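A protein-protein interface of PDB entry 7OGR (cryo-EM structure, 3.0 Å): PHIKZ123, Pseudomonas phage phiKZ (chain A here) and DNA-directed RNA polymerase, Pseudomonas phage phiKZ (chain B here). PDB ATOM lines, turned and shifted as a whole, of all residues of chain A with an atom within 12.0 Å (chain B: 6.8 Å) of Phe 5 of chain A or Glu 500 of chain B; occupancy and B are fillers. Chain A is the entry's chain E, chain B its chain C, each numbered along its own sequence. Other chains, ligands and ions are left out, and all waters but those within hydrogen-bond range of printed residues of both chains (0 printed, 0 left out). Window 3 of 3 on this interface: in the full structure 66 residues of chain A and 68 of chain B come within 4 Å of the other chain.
NZ of Lys 9 of chain A is in salt-bridge range of OE2 of Glu 500 of chain B (3.6 Å).
The side-chain carboxylate (OD2) of Asp 3 of chain A sits at hydrogen-bond distance from the backbone NH (N) of Phe 5 of chain A, 3.1 Å away. The side-chain amino group (NZ) of Lys 9 of chain A is in salt-bridge range of the side-chain carboxylate (OE1) of Glu 12 of chain A.
Asp 3 of chain A touches His 501 of chain B (OD2 to NE2, 3.7 Å). OD1 of Asp 3 of chain A touches CA of His 507 of chain B (3.4 Å). Phe 5 of chain A touches Lys 497 of chain B (CE2 to O, 3.8 Å). Phe 5 of chain A touches Glu 500 of chain B. Phe 5 of chain A touches His 501 of chain B. CE1 of Phe 5 of chain A touches CD of Pro 502 of chain B, at 3.6 Å. Leu 6 of chain A touches Met 498 of chain B (CD1 to CE, 3.8 Å). Lys 9 of chain A touches Lys 497 of chain B (CG to O, 3.7 Å). Asn 13 of chain A touches Lys 497 of chain B.
Pro 2 of chain A touches none of the printed residues of chain B. Of chain B, only Lys 497 (3.8 Å), Glu 500 (3.6 Å), His 501 (3.4 Å) and Pro 502 (3.6 Å) come within 4 Å of Phe 5 of chain A. Of the printed residues of chain B, Leu 6 of chain A touches Met 498. Of the printed residues of chain B, Lys 9 of chain A touches Lys 497 and Glu 500. Of the printed residues of chain B, Asn 13 of chain A touches Lys 497 (3.4 Å). Ser 496 of chain B touches none of the printed residues of chain A. Of chain A, only Phe 5, Lys 9 and Asn 13 come within 4 Å of Lys 497 of chain B. Met 498 of chain B touches just one residue of chain A: Leu 6 (3.8 Å). No residue of chain A comes within 4 Å of Met 499 of chain B. Glu 500 of chain B touches just these residues of chain A: Phe 5 and Lys 9. The nearest residue of chain B that does not touch Phe 5 of chain A is Met 498 of chain B (4.8 Å). The nearest printed residue of chain B that does not touch Asn 13 of chain A is Ser 496 of chain B (7.0 Å).
Printed residues of chain B that touch a printed residue of chain A: Lys 497, Met 498, Glu 500, His 501, Pro 502 and His 507. Hydrophobic or aromatic side chains of chain A within 4 Å of the printed part of chain B: Phe 5 and Leu 6. Along chain A the printed residues that touch a printed residue of chain B span positions 3 to 13. Among the printed residues, 10 pairs touch across the chains. Among the printed residues, Asp or Glu carboxylates within 4 Å of a Lys or Arg side-chain nitrogen of the other chain: Lys 9 of chain A with Glu 500 of chain B (3.6 Å).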
ATOM      1  N   PRO A   2     -34.042  14.900 -15.802  1.00  0.00           N
ATOM      2  CA  PRO A   2     -32.608  14.900 -16.113  1.00  0.00           C
ATOM      3  C   PRO A   2     -31.745  14.578 -14.897  1.00  0.00           C
ATOM      4  O   PRO A   2     -32.229  14.633 -13.766  1.00  0.00           O
ATOM      5  CB  PRO A   2     -32.352  16.331 -16.597  1.00  0.00           C
ATOM      6  CG  PRO A   2     -33.679  16.825 -17.056  1.00  0.00           C
ATOM      7  CD  PRO A   2     -34.689  16.172 -16.165  1.00  0.00           C
ATOM      8  N   ASP A   3     -30.483  14.241 -15.139  1.00  0.00           N
ATOM      9  CA  ASP A   3     -29.567  13.943 -14.048  1.00  0.00           C
ATOM     10  C   ASP A   3     -29.184  15.233 -13.322  1.00  0.00           C
ATOM     11  O   ASP A   3     -28.934  16.253 -13.969  1.00  0.00           O
ATOM     12  CB  ASP A   3     -28.317  13.243 -14.583  1.00  0.00           C
ATOM     13  CG  ASP A   3     -27.489  12.607 -13.488  1.00  0.00           C
ATOM     14  OD1 ASP A   3     -27.835  11.490 -13.052  1.00  0.00           O
ATOM     15  OD2 ASP A   3     -26.490  13.220 -13.063  1.00  0.00           O
ATOM     16  N   PRO A   4     -29.147  15.222 -11.984  1.00  0.00           N
ATOM     17  CA  PRO A   4     -28.837  16.464 -11.253  1.00  0.00           C
ATOM     18  C   PRO A   4     -27.394  16.917 -11.400  1.00  0.00           C
ATOM     19  O   PRO A   4     -27.134  18.125 -11.345  1.00  0.00           O
ATOM     20  CB  PRO A   4     -29.169  16.110  -9.795  1.00  0.00           C
ATOM     21  CG  PRO A   4     -30.011  14.873  -9.864  1.00  0.00           C
ATOM     22  CD  PRO A   4     -29.556  14.135 -11.079  1.00  0.00           C
ATOM     23  N   PHE A   5     -26.450  15.989 -11.589  1.00  0.00           N
ATOM     24  CA  PHE A   5     -25.065  16.381 -11.833  1.00  0.00           C
ATOM     25  C   PHE A   5     -24.909  17.043 -13.197  1.00  0.00           C
ATOM     26  O   PHE A   5     -24.081  17.951 -13.356  1.00  0.00           O
ATOM     27  CB  PHE A   5     -24.154  15.158 -11.719  1.00  0.00           C
ATOM     28  CG  PHE A   5     -22.690  15.486 -11.697  1.00  0.00           C
ATOM     29  CD1 PHE A   5     -22.076  15.879 -10.517  1.00  0.00           C
ATOM     30  CD2 PHE A   5     -21.921  15.383 -12.847  1.00  0.00           C
ATOM     31  CE1 PHE A   5     -20.725  16.177 -10.486  1.00  0.00           C
ATOM     32  CE2 PHE A   5     -20.569  15.677 -12.824  1.00  0.00           C
ATOM     33  CZ  PHE A   5     -19.971  16.072 -11.642  1.00  0.00           C
ATOM     34  N   LEU A   6     -25.721  16.628 -14.175  1.00  0.00           N
ATOM     35  CA  LEU A   6     -25.714  17.272 -15.484  1.00  0.00           C
ATOM     36  C   LEU A   6     -26.227  18.705 -15.397  1.00  0.00           C
ATOM     37  O   LEU A   6     -25.625  19.614 -15.979  1.00  0.00           O
ATOM     38  CB  LEU A   6     -26.553  16.457 -16.470  1.00  0.00           C
ATOM     39  CG  LEU A   6     -26.830  17.067 -17.847  1.00  0.00           C
ATOM     40  CD1 LEU A   6     -25.540  17.278 -18.625  1.00  0.00           C
ATOM     41  CD2 LEU A   6     -27.796  16.193 -18.632  1.00  0.00           C
ATOM     42  N   ILE A   7     -27.316  18.926 -14.655  1.00  0.00           N
ATOM     43  CA  ILE A   7     -27.842  20.276 -14.460  1.00  0.00           C
ATOM     44  C   ILE A   7     -26.867  21.120 -13.644  1.00  0.00           C
ATOM     45  O   ILE A   7     -26.730  22.326 -13.885  1.00  0.00           O
ATOM     46  CB  ILE A   7     -29.238  20.207 -13.806  1.00  0.00           C
ATOM     47  CG1 ILE A   7     -30.145  19.257 -14.591  1.00  0.00           C
ATOM     48  CG2 ILE A   7     -29.889  21.584 -13.731  1.00  0.00           C
ATOM     49  CD1 ILE A   7     -30.468  19.730 -15.995  1.00  0.00           C
ATOM     50  N   GLU A   8     -26.139  20.495 -12.711  1.00  0.00           N
ATOM     51  CA  GLU A   8     -25.105  21.200 -11.957  1.00  0.00           C
ATOM     52  C   GLU A   8     -23.959  21.653 -12.860  1.00  0.00           C
ATOM     53  O   GLU A   8     -23.469  22.780 -12.729  1.00  0.00           O
ATOM     54  CB  GLU A   8     -24.582  20.302 -10.836  1.00  0.00           C
ATOM     55  CG  GLU A   8     -23.576  20.966  -9.912  1.00  0.00           C
ATOM     56  CD  GLU A   8     -23.421  20.227  -8.598  1.00  0.00           C
ATOM     57  OE1 GLU A   8     -24.426  19.676  -8.103  1.00  0.00           O
ATOM     58  OE2 GLU A   8     -22.294  20.196  -8.062  1.00  0.00           O
ATOM     59  N   LYS A   9     -23.540  20.802 -13.802  1.00  0.00           N
ATOM     60  CA  LYS A   9     -22.465  21.196 -14.709  1.00  0.00           C
ATOM     61  C   LYS A   9     -22.920  22.218 -15.746  1.00  0.00           C
ATOM     62  O   LYS A   9     -22.127  23.083 -16.144  1.00  0.00           O
ATOM     63  CB  LYS A   9     -21.878  19.963 -15.398  1.00  0.00           C
ATOM     64  CG  LYS A   9     -20.948  19.156 -14.508  1.00  0.00           C
ATOM     65  CD  LYS A   9     -19.827  20.032 -13.961  1.00  0.00           C
ATOM     66  CE  LYS A   9     -18.986  19.296 -12.933  1.00  0.00           C
ATOM     67  NZ  LYS A   9     -17.917  20.164 -12.366  1.00  0.00           N
ATOM     68  N   ILE A  10     -24.189  22.158 -16.170  1.00  0.00           N
ATOM     69  CA  ILE A  10     -24.722  23.204 -17.041  1.00  0.00           C
ATOM     70  C   ILE A  10     -24.821  24.524 -16.281  1.00  0.00           C
ATOM     71  O   ILE A  10     -24.561  25.594 -16.847  1.00  0.00           O
ATOM     72  CB  ILE A  10     -26.081  22.769 -17.637  1.00  0.00           C
ATOM     73  CG1 ILE A  10     -25.909  21.536 -18.522  1.00  0.00           C
ATOM     74  CG2 ILE A  10     -26.709  23.862 -18.494  1.00  0.00           C
ATOM     75  CD1 ILE A  10     -27.218  20.896 -18.937  1.00  0.00           C
ATOM     76  N   ARG A  11     -25.121  24.468 -14.978  1.00  0.00           N
ATOM     77  CA  ARG A  11     -25.155  25.678 -14.162  1.00  0.00           C
ATOM     78  C   ARG A  11     -23.762  26.266 -13.974  1.00  0.00           C
ATOM     79  O   ARG A  11     -23.591  27.491 -14.005  1.00  0.00           O
ATOM     80  CB  ARG A  11     -25.793  25.373 -12.805  1.00  0.00           C
ATOM     81  CG  ARG A  11     -26.328  26.595 -12.074  1.00  0.00           C
ATOM     82  CD  ARG A  11     -27.202  27.441 -12.981  1.00  0.00           C
ATOM     83  NE  ARG A  11     -27.546  28.721 -12.374  1.00  0.00           N
ATOM     84  CZ  ARG A  11     -27.802  29.826 -13.065  1.00  0.00           C
ATOM     85  NH1 ARG A  11     -27.754  29.808 -14.390  1.00  0.00           N
ATOM     86  NH2 ARG A  11     -28.103  30.950 -12.432  1.00  0.00           N
ATOM     87  N   GLU A  12     -22.754  25.413 -13.780  1.00  0.00           N
ATOM     88  CA  GLU A  12     -21.383  25.904 -13.677  1.00  0.00           C
ATOM     89  C   GLU A  12     -20.825  26.378 -15.015  1.00  0.00           C
ATOM     90  O   GLU A  12     -19.862  27.153 -15.024  1.00  0.00           O
ATOM     91  CB  GLU A  12     -20.460  24.832 -13.094  1.00  0.00           C
ATOM     92  CG  GLU A  12     -20.812  24.392 -11.685  1.00  0.00           C
ATOM     93  CD  GLU A  12     -19.976  23.215 -11.219  1.00  0.00           C
ATOM     94  OE1 GLU A  12     -19.162  22.707 -12.018  1.00  0.00           O
ATOM     95  OE2 GLU A  12     -20.135  22.796 -10.053  1.00  0.00           O
ATOM     96  N   ASN A  13     -21.396  25.944 -16.140  1.00  0.00           N
ATOM     97  CA  ASN A  13     -20.915  26.364 -17.451  1.00  0.00           C
ATOM     98  C   ASN A  13     -21.794  27.425 -18.106  1.00  0.00           C
ATOM     99  O   ASN A  13     -21.658  27.669 -19.309  1.00  0.00           O
ATOM    100  CB  ASN A  13     -20.784  25.155 -18.381  1.00  0.00           C
ATOM    101  CG  ASN A  13     -19.549  25.228 -19.260  1.00  0.00           C
ATOM    102  OD1 ASN A  13     -18.652  26.037 -19.025  1.00  0.00           O
ATOM    103  ND2 ASN A  13     -19.500  24.381 -20.282  1.00  0.00           N
ATOM    104  N   THR A  14     -22.691  28.064 -17.352  1.00  0.00           N
ATOM    105  CA  THR A  14     -23.575  29.078 -17.916  1.00  0.00           C
ATOM    106  C   THR A  14     -23.237  30.455 -17.366  1.00  0.00           C
ATOM    107  O   THR A  14     -23.154  30.620 -16.142  1.00  0.00           O
ATOM    108  CB  THR A  14     -25.042  28.750 -17.612  1.00  0.00           C
ATOM    109  OG1 THR A  14     -25.353  27.443 -18.112  1.00  0.00           O
ATOM    110  CG2 THR A  14     -25.965  29.764 -18.260  1.00  0.00           C
ATOM    111  N   HIS B 495     -18.887  15.032 -22.805  1.00  0.00           N
ATOM    112  CA  HIS B 495     -17.884  13.998 -22.576  1.00  0.00           C
ATOM    113  C   HIS B 495     -16.732  14.513 -21.722  1.00  0.00           C
ATOM    114  O   HIS B 495     -16.120  13.738 -20.980  1.00  0.00           O
ATOM    115  CB  HIS B 495     -17.368  13.465 -23.912  1.00  0.00           C
ATOM    116  CG  HIS B 495     -16.484  12.264 -23.785  1.00  0.00           C
ATOM    117  ND1 HIS B 495     -15.109  12.352 -23.747  1.00  0.00           N
ATOM    118  CD2 HIS B 495     -16.780  10.947 -23.680  1.00  0.00           C
ATOM    119  CE1 HIS B 495     -14.596  11.140 -23.630  1.00  0.00           C
ATOM    120  NE2 HIS B 495     -15.589  10.270 -23.587  1.00  0.00           N
ATOM    121  N   SER B 496     -16.432  15.810 -21.801  1.00  0.00           N
ATOM    122  CA  SER B 496     -15.440  16.385 -20.901  1.00  0.00           C
ATOM    123  C   SER B 496     -16.004  16.645 -19.508  1.00  0.00           C
ATOM    124  O   SER B 496     -15.259  16.576 -18.524  1.00  0.00           O
ATOM    125  CB  SER B 496     -14.883  17.684 -21.484  1.00  0.00           C
ATOM    126  OG  SER B 496     -15.926  18.571 -21.842  1.00  0.00           O
ATOM    127  N   LYS B 497     -17.301  16.939 -19.396  1.00  0.00           N
ATOM    128  CA  LYS B 497     -17.885  17.359 -18.127  1.00  0.00           C
ATOM    129  C   LYS B 497     -18.535  16.233 -17.328  1.00  0.00           C
ATOM    130  O   LYS B 497     -19.024  16.492 -16.225  1.00  0.00           O
ATOM    131  CB  LYS B 497     -18.908  18.476 -18.356  1.00  0.00           C
ATOM    132  CG  LYS B 497     -18.284  19.816 -18.704  1.00  0.00           C
ATOM    133  CD  LYS B 497     -18.971  20.950 -17.966  1.00  0.00           C
ATOM    134  CE  LYS B 497     -18.122  22.208 -17.991  1.00  0.00           C
ATOM    135  NZ  LYS B 497     -18.460  23.130 -16.872  1.00  0.00           N
ATOM    136  N   MET B 498     -18.565  14.995 -17.838  1.00  0.00           N
ATOM    137  CA  MET B 498     -19.009  13.901 -16.981  1.00  0.00           C
ATOM    138  C   MET B 498     -18.109  12.673 -17.085  1.00  0.00           C
ATOM    139  O   MET B 498     -18.523  11.574 -16.696  1.00  0.00           O
ATOM    140  CB  MET B 498     -20.475  13.515 -17.250  1.00  0.00           C
ATOM    141  CG  MET B 498     -20.788  12.922 -18.606  1.00  0.00           C
ATOM    142  SD  MET B 498     -22.557  12.625 -18.758  1.00  0.00           S
ATOM    143  CE  MET B 498     -23.167  14.306 -18.849  1.00  0.00           C
ATOM    144  N   MET B 499     -16.878  12.831 -17.577  1.00  0.00           N
ATOM    145  CA  MET B 499     -15.836  11.874 -17.226  1.00  0.00           C
ATOM    146  C   MET B 499     -15.401  12.062 -15.778  1.00  0.00           C
ATOM    147  O   MET B 499     -14.858  11.135 -15.164  1.00  0.00           O
ATOM    148  CB  MET B 499     -14.636  12.010 -18.164  1.00  0.00           C
ATOM    149  CG  MET B 499     -14.718  11.150 -19.413  1.00  0.00           C
ATOM    150  SD  MET B 499     -13.140  11.036 -20.278  1.00  0.00           S
ATOM    151  CE  MET B 499     -12.936  12.718 -20.859  1.00  0.00           C
ATOM    152  N   GLU B 500     -15.626  13.253 -15.229  1.00  0.00           N
ATOM    153  CA  GLU B 500     -15.370  13.594 -13.830  1.00  0.00           C
ATOM    154  C   GLU B 500     -16.604  13.359 -12.955  1.00  0.00           C
ATOM    155  O   GLU B 500     -16.970  14.172 -12.105  1.00  0.00           O
ATOM    156  CB  GLU B 500     -14.891  15.043 -13.759  1.00  0.00           C
ATOM    157  CG  GLU B 500     -15.839  16.062 -14.423  1.00  0.00           C
ATOM    158  CD  GLU B 500     -15.298  17.479 -14.408  1.00  0.00           C
ATOM    159  OE1 GLU B 500     -14.163  17.683 -13.930  1.00  0.00           O
ATOM    160  OE2 GLU B 500     -16.017  18.392 -14.868  1.00  0.00           O
ATOM    161  N   HIS B 501     -17.232  12.194 -13.129  1.00  0.00           N
ATOM    162  CA  HIS B 501     -18.536  11.924 -12.538  1.00  0.00           C
ATOM    163  C   HIS B 501     -18.393  11.106 -11.267  1.00  0.00           C
ATOM    164  O   HIS B 501     -17.881   9.977 -11.324  1.00  0.00           O
ATOM    165  CB  HIS B 501     -19.423  11.183 -13.533  1.00  0.00           C
ATOM    166  CG  HIS B 501     -20.890  11.356 -13.281  1.00  0.00           C
ATOM    167  ND1 HIS B 501     -21.554  10.699 -12.268  1.00  0.00           N
ATOM    168  CD2 HIS B 501     -21.821  12.105 -13.917  1.00  0.00           C
ATOM    169  CE1 HIS B 501     -22.830  11.041 -12.286  1.00  0.00           C
ATOM    170  NE2 HIS B 501     -23.018  11.894 -13.276  1.00  0.00           N
ATOM    171  N   PRO B 502     -18.817  11.618 -10.111  1.00  0.00           N
ATOM    172  CA  PRO B 502     -18.964  10.765  -8.927  1.00  0.00           C
ATOM    173  C   PRO B 502     -20.341  10.119  -8.888  1.00  0.00           C
ATOM    174  O   PRO B 502     -21.333  10.693  -9.345  1.00  0.00           O
ATOM    175  CB  PRO B 502     -18.782  11.751  -7.766  1.00  0.00           C
ATOM    176  CG  PRO B 502     -19.271  13.054  -8.308  1.00  0.00           C
ATOM    177  CD  PRO B 502     -19.046  13.041  -9.802  1.00  0.00           C
ATOM    178  N   HIS B 507     -26.541   8.044 -12.729  1.00  0.00           N
ATOM    179  CA  HIS B 507     -26.723   8.504 -14.103  1.00  0.00           C
ATOM    180  C   HIS B 507     -27.414   7.447 -14.953  1.00  0.00           C
ATOM    181  O   HIS B 507     -28.331   7.764 -15.721  1.00  0.00           O
ATOM    182  CB  HIS B 507     -25.373   8.882 -14.712  1.00  0.00           C
ATOM    183  CG  HIS B 507     -25.481   9.520 -16.062  1.00  0.00           C
ATOM    184  ND1 HIS B 507     -26.211  10.666 -16.289  1.00  0.00           N
ATOM    185  CD2 HIS B 507     -24.951   9.169 -17.258  1.00  0.00           C
ATOM    186  CE1 HIS B 507     -26.126  10.995 -17.566  1.00  0.00           C
ATOM    187  NE2 HIS B 507     -25.367  10.103 -18.176  1.00  0.00           N
